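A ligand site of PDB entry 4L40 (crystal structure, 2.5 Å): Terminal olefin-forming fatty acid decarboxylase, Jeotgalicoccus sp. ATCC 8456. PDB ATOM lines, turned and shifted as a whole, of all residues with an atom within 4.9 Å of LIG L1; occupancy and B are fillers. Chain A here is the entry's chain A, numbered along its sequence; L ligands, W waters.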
ATOM      1  N   TYR A  59      16.360 -18.696 -23.122  1.00  0.00           N
ATOM      2  CA  TYR A  59      15.311 -18.277 -24.048  1.00  0.00           C
ATOM      3  C   TYR A  59      15.717 -17.037 -24.841  1.00  0.00           C
ATOM      4  O   TYR A  59      14.883 -16.347 -25.400  1.00  0.00           O
ATOM      5  CB  TYR A  59      14.006 -18.030 -23.294  1.00  0.00           C
ATOM      6  CG  TYR A  59      13.362 -19.287 -22.807  1.00  0.00           C
ATOM      7  CD1 TYR A  59      12.745 -20.161 -23.687  1.00  0.00           C
ATOM      8  CD2 TYR A  59      13.334 -19.601 -21.460  1.00  0.00           C
ATOM      9  CE1 TYR A  59      12.142 -21.313 -23.259  1.00  0.00           C
ATOM     10  CE2 TYR A  59      12.724 -20.773 -21.019  1.00  0.00           C
ATOM     11  CZ  TYR A  59      12.143 -21.629 -21.946  1.00  0.00           C
ATOM     12  OH  TYR A  59      11.516 -22.776 -21.515  1.00  0.00           O
ATOM     13  N   ARG A  66      17.084 -24.718 -30.122  1.00  0.00           N
ATOM     14  CA  ARG A  66      16.282 -25.832 -29.571  1.00  0.00           C
ATOM     15  C   ARG A  66      16.130 -26.989 -30.571  1.00  0.00           C
ATOM     16  O   ARG A  66      16.209 -28.148 -30.204  1.00  0.00           O
ATOM     17  CB  ARG A  66      14.887 -25.326 -29.140  1.00  0.00           C
ATOM     18  CG  ARG A  66      14.918 -24.265 -28.032  1.00  0.00           C
ATOM     19  CD  ARG A  66      15.536 -24.798 -26.726  1.00  0.00           C
ATOM     20  NE  ARG A  66      14.699 -25.804 -26.081  1.00  0.00           N
ATOM     21  CZ  ARG A  66      13.595 -25.522 -25.400  1.00  0.00           C
ATOM     22  NH1 ARG A  66      13.203 -24.250 -25.228  1.00  0.00           N
ATOM     23  NH2 ARG A  66      12.888 -26.520 -24.867  1.00  0.00           N
ATOM     24  N   ILE A  84       5.641 -29.119 -33.360  1.00  0.00           N
ATOM     25  CA  ILE A  84       6.018 -27.736 -33.019  1.00  0.00           C
ATOM     26  C   ILE A  84       7.289 -27.648 -32.143  1.00  0.00           C
ATOM     27  O   ILE A  84       8.206 -26.881 -32.416  1.00  0.00           O
ATOM     28  CB  ILE A  84       4.805 -27.010 -32.359  1.00  0.00           C
ATOM     29  CG1 ILE A  84       5.161 -25.576 -31.974  1.00  0.00           C
ATOM     30  CG2 ILE A  84       4.263 -27.772 -31.172  1.00  0.00           C
ATOM     31  CD1 ILE A  84       4.413 -24.572 -32.863  1.00  0.00           C
ATOM     32  N   HIS A  85       7.380 -28.537 -31.153  1.00  0.00           N
ATOM     33  CA  HIS A  85       8.563 -28.655 -30.299  1.00  0.00           C
ATOM     34  C   HIS A  85       9.907 -28.823 -31.018  1.00  0.00           C
ATOM     35  O   HIS A  85      10.962 -28.549 -30.399  1.00  0.00           O
ATOM     36  CB  HIS A  85       8.418 -29.851 -29.364  1.00  0.00           C
ATOM     37  CG  HIS A  85       7.115 -29.904 -28.628  1.00  0.00           C
ATOM     38  ND1 HIS A  85       5.925 -30.263 -29.235  1.00  0.00           N
ATOM     39  CD2 HIS A  85       6.827 -29.683 -27.325  1.00  0.00           C
ATOM     40  CE1 HIS A  85       4.961 -30.239 -28.334  1.00  0.00           C
ATOM     41  NE2 HIS A  85       5.472 -29.891 -27.164  1.00  0.00           N
ATOM     42  N   HIS A  92       8.657 -21.797 -36.884  1.00  0.00           N
ATOM     43  CA  HIS A  92       8.125 -21.981 -35.526  1.00  0.00           C
ATOM     44  C   HIS A  92       7.164 -20.861 -35.060  1.00  0.00           C
ATOM     45  O   HIS A  92       6.091 -21.161 -34.534  1.00  0.00           O
ATOM     46  CB  HIS A  92       9.272 -22.153 -34.501  1.00  0.00           C
ATOM     47  CG  HIS A  92       8.813 -22.047 -33.084  1.00  0.00           C
ATOM     48  ND1 HIS A  92       8.996 -20.911 -32.319  1.00  0.00           N
ATOM     49  CD2 HIS A  92       8.121 -22.911 -32.311  1.00  0.00           C
ATOM     50  CE1 HIS A  92       8.447 -21.090 -31.128  1.00  0.00           C
ATOM     51  NE2 HIS A  92       7.916 -22.300 -31.103  1.00  0.00           N
ATOM     52  N   LYS A  96       3.430 -21.411 -33.968  1.00  0.00           N
ATOM     53  CA  LYS A  96       3.134 -21.167 -32.602  1.00  0.00           C
ATOM     54  C   LYS A  96       1.947 -20.235 -32.569  1.00  0.00           C
ATOM     55  O   LYS A  96       1.113 -20.350 -31.663  1.00  0.00           O
ATOM     56  CB  LYS A  96       4.347 -20.548 -31.878  1.00  0.00           C
ATOM     57  CG  LYS A  96       4.154 -20.313 -30.389  1.00  0.00           C
ATOM     58  CD  LYS A  96       3.770 -21.604 -29.663  1.00  0.00           C
ATOM     59  CE  LYS A  96       3.755 -21.448 -28.160  1.00  0.00           C
ATOM     60  NZ  LYS A  96       5.127 -21.605 -27.595  1.00  0.00           N
ATOM     61  N   PHE A  99      -1.296 -22.240 -32.399  1.00  0.00           N
ATOM     62  CA  PHE A  99      -1.525 -22.744 -31.073  1.00  0.00           C
ATOM     63  C   PHE A  99      -2.131 -21.684 -30.151  1.00  0.00           C
ATOM     64  O   PHE A  99      -3.229 -21.842 -29.606  1.00  0.00           O
ATOM     65  CB  PHE A  99      -0.224 -23.325 -30.488  1.00  0.00           C
ATOM     66  CG  PHE A  99       0.072 -24.739 -30.951  1.00  0.00           C
ATOM     67  CD1 PHE A  99       0.782 -24.970 -32.108  1.00  0.00           C
ATOM     68  CD2 PHE A  99      -0.385 -25.826 -30.261  1.00  0.00           C
ATOM     69  CE1 PHE A  99       1.032 -26.221 -32.530  1.00  0.00           C
ATOM     70  CE2 PHE A  99      -0.095 -27.093 -30.695  1.00  0.00           C
ATOM     71  CZ  PHE A  99       0.593 -27.289 -31.826  1.00  0.00           C
ATOM     72  N   MET A 103      -6.198 -19.870 -27.652  1.00  0.00           N
ATOM     73  CA  MET A 103      -6.267 -19.466 -26.243  1.00  0.00           C
ATOM     74  C   MET A 103      -6.985 -18.128 -26.004  1.00  0.00           C
ATOM     75  O   MET A 103      -6.490 -17.277 -25.243  1.00  0.00           O
ATOM     76  CB  MET A 103      -4.854 -19.448 -25.642  1.00  0.00           C
ATOM     77  CG  MET A 103      -4.060 -20.675 -25.909  1.00  0.00           C
ATOM     78  SD  MET A 103      -4.843 -22.209 -25.355  1.00  0.00           S
ATOM     79  CE  MET A 103      -3.683 -23.374 -26.119  1.00  0.00           C
ATOM     80  N   TRP A 149     -12.885 -30.202 -26.026  1.00  0.00           N
ATOM     81  CA  TRP A 149     -12.323 -28.884 -26.123  1.00  0.00           C
ATOM     82  C   TRP A 149     -11.633 -28.690 -27.489  1.00  0.00           C
ATOM     83  O   TRP A 149     -11.768 -27.621 -28.099  1.00  0.00           O
ATOM     84  CB  TRP A 149     -11.354 -28.572 -24.939  1.00  0.00           C
ATOM     85  CG  TRP A 149     -10.807 -27.214 -25.063  1.00  0.00           C
ATOM     86  CD1 TRP A 149     -11.463 -26.049 -24.792  1.00  0.00           C
ATOM     87  CD2 TRP A 149      -9.544 -26.847 -25.608  1.00  0.00           C
ATOM     88  NE1 TRP A 149     -10.646 -24.965 -25.083  1.00  0.00           N
ATOM     89  CE2 TRP A 149      -9.474 -25.437 -25.598  1.00  0.00           C
ATOM     90  CE3 TRP A 149      -8.452 -27.570 -26.078  1.00  0.00           C
ATOM     91  CZ2 TRP A 149      -8.348 -24.729 -26.043  1.00  0.00           C
ATOM     92  CZ3 TRP A 149      -7.319 -26.869 -26.522  1.00  0.00           C
ATOM     93  CH2 TRP A 149      -7.287 -25.467 -26.497  1.00  0.00           C
ATOM     94  N   ASN A 242      -0.989 -32.330 -29.920  1.00  0.00           N
ATOM     95  CA  ASN A 242      -0.178 -31.479 -29.033  1.00  0.00           C
ATOM     96  C   ASN A 242      -1.022 -30.379 -28.385  1.00  0.00           C
ATOM     97  O   ASN A 242      -0.514 -29.570 -27.611  1.00  0.00           O
ATOM     98  CB  ASN A 242       1.051 -30.904 -29.747  1.00  0.00           C
ATOM     99  CG  ASN A 242       2.184 -31.917 -29.856  1.00  0.00           C
ATOM    100  OD1 ASN A 242       2.317 -32.800 -29.007  1.00  0.00           O
ATOM    101  ND2 ASN A 242       2.986 -31.810 -30.895  1.00  0.00           N
ATOM    102  N   THR A 243      -2.306 -30.416 -28.683  1.00  0.00           N
ATOM    103  CA  THR A 243      -3.284 -29.436 -28.264  1.00  0.00           C
ATOM    104  C   THR A 243      -4.145 -30.006 -27.112  1.00  0.00           C
ATOM    105  O   THR A 243      -4.830 -29.262 -26.410  1.00  0.00           O
ATOM    106  CB  THR A 243      -4.069 -29.059 -29.551  1.00  0.00           C
ATOM    107  OG1 THR A 243      -3.727 -27.727 -29.993  1.00  0.00           O
ATOM    108  CG2 THR A 243      -5.532 -29.260 -29.424  1.00  0.00           C
ATOM    109  N   PRO A 246      -1.383 -32.931 -23.771  1.00  0.00           N
ATOM    110  CA  PRO A 246      -0.824 -32.303 -22.557  1.00  0.00           C
ATOM    111  C   PRO A 246      -1.911 -31.802 -21.579  1.00  0.00           C
ATOM    112  O   PRO A 246      -1.651 -31.646 -20.360  1.00  0.00           O
ATOM    113  CB  PRO A 246      -0.006 -31.134 -23.115  1.00  0.00           C
ATOM    114  CG  PRO A 246       0.230 -31.451 -24.558  1.00  0.00           C
ATOM    115  CD  PRO A 246      -1.013 -32.180 -24.990  1.00  0.00           C
ATOM    116  N   LEU A 247      -3.095 -31.520 -22.108  1.00  0.00           N
ATOM    117  CA  LEU A 247      -4.223 -31.160 -21.270  1.00  0.00           C
ATOM    118  C   LEU A 247      -4.582 -32.366 -20.397  1.00  0.00           C
ATOM    119  O   LEU A 247      -4.844 -32.248 -19.201  1.00  0.00           O
ATOM    120  CB  LEU A 247      -5.388 -30.752 -22.158  1.00  0.00           C
ATOM    121  CG  LEU A 247      -6.721 -30.304 -21.573  1.00  0.00           C
ATOM    122  CD1 LEU A 247      -7.546 -29.683 -22.683  1.00  0.00           C
ATOM    123  CD2 LEU A 247      -7.484 -31.390 -20.902  1.00  0.00           C
ATOM    124  N   ALA A 249      -2.653 -34.749 -19.593  1.00  0.00           N
ATOM    125  CA  ALA A 249      -1.534 -34.979 -18.683  1.00  0.00           C
ATOM    126  C   ALA A 249      -1.642 -34.178 -17.385  1.00  0.00           C
ATOM    127  O   ALA A 249      -0.941 -34.454 -16.398  1.00  0.00           O
ATOM    128  CB  ALA A 249      -0.219 -34.639 -19.399  1.00  0.00           C
ATOM    129  N   ILE A 250      -2.522 -33.192 -17.360  1.00  0.00           N
ATOM    130  CA  ILE A 250      -2.852 -32.504 -16.109  1.00  0.00           C
ATOM    131  C   ILE A 250      -3.330 -33.486 -15.057  1.00  0.00           C
ATOM    132  O   ILE A 250      -3.333 -33.153 -13.886  1.00  0.00           O
ATOM    133  CB  ILE A 250      -3.920 -31.403 -16.331  1.00  0.00           C
ATOM    134  CG1 ILE A 250      -3.402 -30.353 -17.295  1.00  0.00           C
ATOM    135  CG2 ILE A 250      -4.236 -30.674 -15.047  1.00  0.00           C
ATOM    136  CD1 ILE A 250      -4.488 -29.514 -17.840  1.00  0.00           C
ATOM    137  N   PHE A 253      -1.154 -33.537 -12.165  1.00  0.00           N
ATOM    138  CA  PHE A 253      -1.281 -32.465 -11.215  1.00  0.00           C
ATOM    139  C   PHE A 253      -2.530 -32.576 -10.396  1.00  0.00           C
ATOM    140  O   PHE A 253      -2.573 -32.064  -9.292  1.00  0.00           O
ATOM    141  CB  PHE A 253      -1.270 -31.099 -11.926  1.00  0.00           C
ATOM    142  CG  PHE A 253       0.085 -30.614 -12.365  1.00  0.00           C
ATOM    143  CD1 PHE A 253       1.234 -30.864 -11.610  1.00  0.00           C
ATOM    144  CD2 PHE A 253       0.218 -29.864 -13.528  1.00  0.00           C
ATOM    145  CE1 PHE A 253       2.471 -30.380 -12.042  1.00  0.00           C
ATOM    146  CE2 PHE A 253       1.457 -29.364 -13.942  1.00  0.00           C
ATOM    147  CZ  PHE A 253       2.585 -29.621 -13.210  1.00  0.00           C
ATOM    148  N   PHE A 291       7.601 -32.575 -12.305  1.00  0.00           N
ATOM    149  CA  PHE A 291       7.095 -33.141 -13.542  1.00  0.00           C
ATOM    150  C   PHE A 291       8.200 -33.023 -14.571  1.00  0.00           C
ATOM    151  O   PHE A 291       8.791 -34.034 -14.928  1.00  0.00           O
ATOM    152  CB  PHE A 291       5.838 -32.390 -13.986  1.00  0.00           C
ATOM    153  CG  PHE A 291       4.995 -33.113 -15.048  1.00  0.00           C
ATOM    154  CD1 PHE A 291       3.625 -33.266 -14.874  1.00  0.00           C
ATOM    155  CD2 PHE A 291       5.557 -33.592 -16.201  1.00  0.00           C
ATOM    156  CE1 PHE A 291       2.860 -33.885 -15.840  1.00  0.00           C
ATOM    157  CE2 PHE A 291       4.756 -34.218 -17.174  1.00  0.00           C
ATOM    158  CZ  PHE A 291       3.422 -34.351 -16.988  1.00  0.00           C
ATOM    159  N   VAL A 292       8.471 -31.786 -15.009  1.00  0.00           N
ATOM    160  CA  VAL A 292       9.486 -31.520 -16.023  1.00  0.00           C
ATOM    161  C   VAL A 292      10.812 -31.265 -15.360  1.00  0.00           C
ATOM    162  O   VAL A 292      10.956 -30.292 -14.650  1.00  0.00           O
ATOM    163  CB  VAL A 292       9.131 -30.312 -16.930  1.00  0.00           C
ATOM    164  CG1 VAL A 292      10.207 -30.114 -18.000  1.00  0.00           C
ATOM    165  CG2 VAL A 292       7.771 -30.531 -17.594  1.00  0.00           C
ATOM    166  N   LEU A 295      15.215 -28.933 -19.788  1.00  0.00           N
ATOM    167  CA  LEU A 295      14.992 -28.843 -21.211  1.00  0.00           C
ATOM    168  C   LEU A 295      16.317 -28.714 -21.944  1.00  0.00           C
ATOM    169  O   LEU A 295      17.187 -27.990 -21.481  1.00  0.00           O
ATOM    170  CB  LEU A 295      14.091 -27.630 -21.537  1.00  0.00           C
ATOM    171  CG  LEU A 295      12.706 -27.792 -20.889  1.00  0.00           C
ATOM    172  CD1 LEU A 295      11.995 -26.424 -20.775  1.00  0.00           C
ATOM    173  CD2 LEU A 295      11.907 -28.833 -21.680  1.00  0.00           C
ATOM    174  N   PRO A 353       7.666 -24.172 -14.588  1.00  0.00           N
ATOM    175  CA  PRO A 353       7.504 -25.629 -14.644  1.00  0.00           C
ATOM    176  C   PRO A 353       7.004 -26.139 -15.995  1.00  0.00           C
ATOM    177  O   PRO A 353       7.129 -27.335 -16.267  1.00  0.00           O
ATOM    178  CB  PRO A 353       6.443 -25.895 -13.570  1.00  0.00           C
ATOM    179  CG  PRO A 353       5.614 -24.655 -13.555  1.00  0.00           C
ATOM    180  CD  PRO A 353       6.601 -23.534 -13.804  1.00  0.00           C
ATOM    181  N   GLN A 354       6.448 -25.239 -16.816  1.00  0.00           N
ATOM    182  CA  GLN A 354       5.990 -25.532 -18.184  1.00  0.00           C
ATOM    183  C   GLN A 354       6.717 -24.630 -19.169  1.00  0.00           C
ATOM    184  O   GLN A 354       6.182 -24.226 -20.199  1.00  0.00           O
ATOM    185  CB  GLN A 354       4.459 -25.367 -18.274  1.00  0.00           C
ATOM    186  CG  GLN A 354       3.735 -26.307 -17.267  1.00  0.00           C
ATOM    187  CD  GLN A 354       2.212 -26.254 -17.291  1.00  0.00           C
ATOM    188  OE1 GLN A 354       1.580 -26.327 -18.343  1.00  0.00           O
ATOM    189  NE2 GLN A 354       1.617 -26.202 -16.103  1.00  0.00           N
ATOM    190  N   GLY A 355       7.968 -24.334 -18.825  1.00  0.00           N
ATOM    191  CA  GLY A 355       8.816 -23.433 -19.596  1.00  0.00           C
ATOM    192  C   GLY A 355       8.838 -21.994 -19.101  1.00  0.00           C
ATOM    193  O   GLY A 355       8.036 -21.560 -18.278  1.00  0.00           O
ATOM    194  N   ASN A 362       9.254 -17.936 -28.123  1.00  0.00           N
ATOM    195  CA  ASN A 362       9.976 -19.059 -27.520  1.00  0.00           C
ATOM    196  C   ASN A 362       9.116 -20.343 -27.495  1.00  0.00           C
ATOM    197  O   ASN A 362       7.921 -20.324 -27.791  1.00  0.00           O
ATOM    198  CB  ASN A 362      10.301 -18.680 -26.051  1.00  0.00           C
ATOM    199  CG  ASN A 362      11.379 -17.568 -25.919  1.00  0.00           C
ATOM    200  OD1 ASN A 362      11.167 -16.561 -25.247  1.00  0.00           O
ATOM    201  ND2 ASN A 362      12.541 -17.791 -26.484  1.00  0.00           N
ATOM    202  N   HIS A 363       9.680 -21.443 -27.044  1.00  0.00           N
ATOM    203  CA  HIS A 363       8.937 -22.714 -27.020  1.00  0.00           C
ATOM    204  C   HIS A 363       8.104 -22.908 -25.716  1.00  0.00           C
ATOM    205  O   HIS A 363       7.713 -24.056 -25.378  1.00  0.00           O
ATOM    206  CB  HIS A 363       9.919 -23.897 -27.155  1.00  0.00           C
ATOM    207  CG  HIS A 363      10.368 -24.164 -28.566  1.00  0.00           C
ATOM    208  ND1 HIS A 363       9.625 -24.923 -29.448  1.00  0.00           N
ATOM    209  CD2 HIS A 363      11.489 -23.798 -29.231  1.00  0.00           C
ATOM    210  CE1 HIS A 363      10.288 -25.020 -30.588  1.00  0.00           C
ATOM    211  NE2 HIS A 363      11.411 -24.346 -30.482  1.00  0.00           N
ATOM    212  N   ARG A 364       7.831 -21.819 -25.007  1.00  0.00           N
ATOM    213  CA  ARG A 364       7.049 -21.912 -23.769  1.00  0.00           C
ATOM    214  C   ARG A 364       5.682 -22.574 -24.047  1.00  0.00           C
ATOM    215  O   ARG A 364       5.060 -22.350 -25.111  1.00  0.00           O
ATOM    216  CB  ARG A 364       6.819 -20.540 -23.156  1.00  0.00           C
ATOM    217  CG  ARG A 364       6.317 -20.568 -21.704  1.00  0.00           C
ATOM    218  CD  ARG A 364       5.845 -19.141 -21.256  1.00  0.00           C
ATOM    219  NE  ARG A 364       5.463 -19.141 -19.868  1.00  0.00           N
ATOM    220  CZ  ARG A 364       6.046 -18.446 -18.907  1.00  0.00           C
ATOM    221  NH1 ARG A 364       6.993 -17.569 -19.171  1.00  0.00           N
ATOM    222  NH2 ARG A 364       5.656 -18.610 -17.652  1.00  0.00           N
ATOM    223  N   CYS A 365       5.262 -23.395 -23.082  1.00  0.00           N
ATOM    224  CA  CYS A 365       3.978 -24.079 -23.113  1.00  0.00           C
ATOM    225  C   CYS A 365       2.821 -23.150 -23.517  1.00  0.00           C
ATOM    226  O   CYS A 365       2.652 -22.067 -22.972  1.00  0.00           O
ATOM    227  CB  CYS A 365       3.668 -24.685 -21.743  1.00  0.00           C
ATOM    228  SG  CYS A 365       2.194 -25.682 -21.719  1.00  0.00           S
ATOM    229  N   ALA A 366       2.050 -23.625 -24.490  1.00  0.00           N
ATOM    230  CA  ALA A 366       0.895 -22.945 -24.997  1.00  0.00           C
ATOM    231  C   ALA A 366      -0.285 -23.038 -24.003  1.00  0.00           C
ATOM    232  O   ALA A 366      -1.227 -22.250 -24.043  1.00  0.00           O
ATOM    233  CB  ALA A 366       0.520 -23.597 -26.312  1.00  0.00           C
ATOM    234  N   GLY A 367      -0.239 -24.029 -23.116  1.00  0.00           N
ATOM    235  CA  GLY A 367      -1.403 -24.430 -22.333  1.00  0.00           C
ATOM    236  C   GLY A 367      -1.290 -24.237 -20.853  1.00  0.00           C
ATOM    237  O   GLY A 367      -1.896 -24.952 -20.068  1.00  0.00           O
ATOM    238  N   ILE A 370      -4.694 -22.839 -19.589  1.00  0.00           N
ATOM    239  CA  ILE A 370      -5.609 -24.007 -19.475  1.00  0.00           C
ATOM    240  C   ILE A 370      -5.225 -24.889 -18.297  1.00  0.00           C
ATOM    241  O   ILE A 370      -6.089 -25.395 -17.582  1.00  0.00           O
ATOM    242  CB  ILE A 370      -5.648 -24.919 -20.774  1.00  0.00           C
ATOM    243  CG1 ILE A 370      -6.379 -24.182 -21.904  1.00  0.00           C
ATOM    244  CG2 ILE A 370      -6.324 -26.269 -20.497  1.00  0.00           C
ATOM    245  CD1 ILE A 370      -6.361 -24.905 -23.223  1.00  0.00           C
ATOM    246  N   THR A 371      -3.938 -25.072 -18.079  1.00  0.00           N
ATOM    247  CA  THR A 371      -3.519 -25.923 -16.943  1.00  0.00           C
ATOM    248  C   THR A 371      -4.001 -25.307 -15.635  1.00  0.00           C
ATOM    249  O   THR A 371      -4.625 -25.967 -14.792  1.00  0.00           O
ATOM    250  CB  THR A 371      -1.999 -26.115 -16.925  1.00  0.00           C
ATOM    251  OG1 THR A 371      -1.579 -26.676 -18.182  1.00  0.00           O
ATOM    252  CG2 THR A 371      -1.589 -27.042 -15.787  1.00  0.00           C
HETATM  253  C1  LIG L   1       5.454 -26.874 -24.364  1.00  0.00           C
HETATM  254  C2  LIG L   1       5.005 -28.598 -19.943  1.00  0.00           C
HETATM  255  C3  LIG L   1       0.178 -28.752 -20.381  1.00  0.00           C
HETATM  256  C4  LIG L   1       0.682 -27.325 -24.934  1.00  0.00           C
HETATM  257  C5  LIG L   1       5.738 -27.297 -23.117  1.00  0.00           C
HETATM  258  C6  LIG L   1       7.072 -27.368 -22.549  1.00  0.00           C
HETATM  259  C7  LIG L   1       6.977 -27.832 -21.299  1.00  0.00           C
HETATM  260  C8  LIG L   1       5.551 -28.062 -21.062  1.00  0.00           C
HETATM  261  C9  LIG L   1       8.188 -28.058 -20.369  1.00  0.00           C
HETATM  262  C10 LIG L   1       8.366 -26.966 -23.275  1.00  0.00           C
HETATM  263  C11 LIG L   1       8.843 -25.583 -22.879  1.00  0.00           C
HETATM  264  C12 LIG L   1      10.015 -25.274 -23.762  1.00  0.00           C
HETATM  265  O1  LIG L   1      10.697 -24.241 -23.520  1.00  0.00           O
HETATM  266  O2  LIG L   1      10.262 -26.055 -24.714  1.00  0.00           O
HETATM  267  C13 LIG L   1       3.677 -28.888 -19.755  1.00  0.00           C
HETATM  268  C14 LIG L   1       3.195 -29.624 -18.613  1.00  0.00           C
HETATM  269  C15 LIG L   1       1.855 -29.690 -18.704  1.00  0.00           C
HETATM  270  C16 LIG L   1       1.445 -28.986 -19.914  1.00  0.00           C
HETATM  271  C17 LIG L   1       4.040 -30.254 -17.497  1.00  0.00           C
HETATM  272  C18 LIG L   1       1.020 -30.431 -17.638  1.00  0.00           C
HETATM  273  C19 LIG L   1      -0.262 -30.678 -17.782  1.00  0.00           C
HETATM  274  C20 LIG L   1      -0.097 -28.293 -21.645  1.00  0.00           C
HETATM  275  C21 LIG L   1      -1.425 -28.039 -22.201  1.00  0.00           C
HETATM  276  C22 LIG L   1      -1.273 -27.659 -23.480  1.00  0.00           C
HETATM  277  C23 LIG L   1       0.143 -27.646 -23.744  1.00  0.00           C
HETATM  278  C24 LIG L   1      -2.731 -28.203 -21.427  1.00  0.00           C
HETATM  279  C25 LIG L   1      -2.316 -27.268 -24.541  1.00  0.00           C
HETATM  280  C26 LIG L   1      -3.595 -27.124 -24.217  1.00  0.00           C
HETATM  281  C27 LIG L   1       2.016 -27.197 -25.214  1.00  0.00           C
HETATM  282  C28 LIG L   1       2.533 -27.026 -26.537  1.00  0.00           C
HETATM  283  C29 LIG L   1       4.027 -26.879 -26.337  1.00  0.00           C
HETATM  284  C30 LIG L   1       4.220 -26.970 -24.915  1.00  0.00           C
HETATM  285  C31 LIG L   1       1.762 -27.007 -27.870  1.00  0.00           C
HETATM  286  C32 LIG L   1       5.145 -26.695 -27.382  1.00  0.00           C
HETATM  287  C33 LIG L   1       5.208 -25.193 -27.618  1.00  0.00           C
HETATM  288  C34 LIG L   1       6.309 -24.843 -28.563  1.00  0.00           C
HETATM  289  O3  LIG L   1       6.349 -23.640 -28.930  1.00  0.00           O
HETATM  290  O4  LIG L   1       7.128 -25.722 -28.944  1.00  0.00           O
HETATM  291  N1  LIG L   1       4.813 -27.702 -22.185  1.00  0.00           N
HETATM  292  N2  LIG L   1       2.597 -28.507 -20.535  1.00  0.00           N
HETATM  293  N3  LIG L   1       0.841 -28.002 -22.614  1.00  0.00           N
HETATM  294  N4  LIG L   1       3.004 -27.136 -24.252  1.00  0.00           N
HETATM  295 FE1  LIG L   1       2.780 -27.779 -22.399  1.00  0.00          FE
HETATM  296  O1  LG2 L   2       3.336 -32.920 -23.709  1.00  0.00           O
HETATM  297  C1  LG2 L   2       2.668 -33.454 -22.781  1.00  0.00           C
HETATM  298  O2  LG2 L   2       2.042 -34.525 -22.886  1.00  0.00           O
HETATM  299  C2  LG2 L   2       2.550 -32.784 -21.433  1.00  0.00           C
HETATM  300  C3  LG2 L   2       3.785 -33.088 -20.637  1.00  0.00           C
HETATM  301  C4  LG2 L   2       4.960 -32.295 -21.167  1.00  0.00           C
HETATM  302  C5  LG2 L   2       6.133 -33.208 -21.407  1.00  0.00           C
HETATM  303  C6  LG2 L   2       7.248 -33.012 -20.386  1.00  0.00           C
HETATM  304  C7  LG2 L   2       8.554 -32.708 -21.109  1.00  0.00           C
HETATM  305  C8  LG2 L   2       9.707 -33.571 -20.659  1.00  0.00           C
HETATM  306  C9  LG2 L   2      10.941 -33.244 -21.520  1.00  0.00           C
HETATM  307  C10 LG2 L   2      12.222 -33.787 -20.895  1.00  0.00           C
HETATM  308  C11 LG2 L   2      13.429 -33.444 -21.762  1.00  0.00           C
HETATM  309  C12 LG2 L   2      14.404 -34.607 -21.915  1.00  0.00           C
HETATM  310  C13 LG2 L   2      15.756 -34.114 -22.421  1.00  0.00           C
HETATM  311  C14 LG2 L   2      16.846 -34.451 -21.424  1.00  0.00           C
HETATM  312  C15 LG2 L   2      18.105 -33.637 -21.679  1.00  0.00           C
HETATM  313  C16 LG2 L   2      19.265 -34.091 -20.810  1.00  0.00           C
HETATM  314  C17 LG2 L   2      19.983 -33.173 -20.169  1.00  0.00           C
HETATM  315  C18 LG2 L   2      21.150 -33.524 -19.293  1.00  0.00           C
HETATM  316  C19 LG2 L   2      20.926 -33.130 -17.898  1.00  0.00           C
HETATM  317  C20 LG2 L   2      20.800 -32.814 -16.672  1.00  0.00           C
HETATM  318  O   HOH W   1       3.841 -30.315 -24.231  1.00  0.00           O
HETATM  319  O   HOH W   2       2.472 -30.156 -26.557  1.00  0.00           O
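The side-chain amino group of Lys 96 is in salt-bridge range of an oxygen (O3) of LIG L1 (2.7 Å).
A ring nitrogen (NE2) of His 92 is in hydrogen-bond range of an oxygen (O3) of LIG L1 (3.0 Å).
O1 of LIG L1 is in hydrogen-bond range of OH of Tyr 59 (2.6 Å).
NH2 of Arg 66 is in salt-bridge range of O2 of LIG L1, 2.7 Å away.
ND1 of His 363 lies within hydrogen-bond range of O4 of LIG L1 (2.7 Å).
SG of Cys 365 is bound to FE1 of LIG L1 (2.3 Å).
The side-chain amide oxygen (OE1) of Gln 354 lies within hydrogen-bond range of the side-chain hydroxyl (OG1) of Thr 371, at 3.2 Å.
NZ of Lys 96 lies within hydrogen-bond range of O of Arg 364, 2.6 Å away.
The backbone NH (N) of Gly 367 sits close to the side-chain sulfur (SG) of Cys 365, at 3.3 Å.
The side-chain amino group (NZ) of Lys 96 sits at hydrogen-bond distance from the backbone carbonyl oxygen (O) of Asn 362 (3.1 Å).
OG1 of Thr 371 is in hydrogen-bond range of O of Gly 367, at 2.6 Å.
O of Tyr 59 sits at hydrogen-bond distance from ND2 of Asn 362 (3.0 Å).
The backbone NH of Cys 365 sits close to the backbone carbonyl oxygen of Gln 354 (3.1 Å).
The side-chain amide oxygen of Gln 354 lies close to a nitrogen (N2) of LIG L1 (3.3 Å).
Merely in contact with LIG L1: Ile 84, His 85, Phe 99, Asn 242, Thr 243, Pro 246, Leu 247, Ala 249, Ile 250, Phe 253, Phe 291, Val 292, Leu 295, Gly 355, Asn 362, Arg 364, Ala 366, Gly 367, Ile 370 and Thr 371.
Hydrophobic or aromatic side chains within 4 Å of LIG L1: Tyr 59, Ile 84, His 85, His 92, Phe 99, Pro 246, Leu 247, Ile 250, Phe 253, Phe 291, Val 292, Leu 295, His 363, Ala 366 and Ile 370.
Of the 30 residues printed, 27 come within 4 Å of LIG L1.
Water W2 bridges NE2 of His 85 (3.1 Å) and O of Asn 242 (3.2 Å).
Water W1 bridges O1 of LG2 L2 (2.7 Å) and NE2 of His 85 (3.4 Å).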
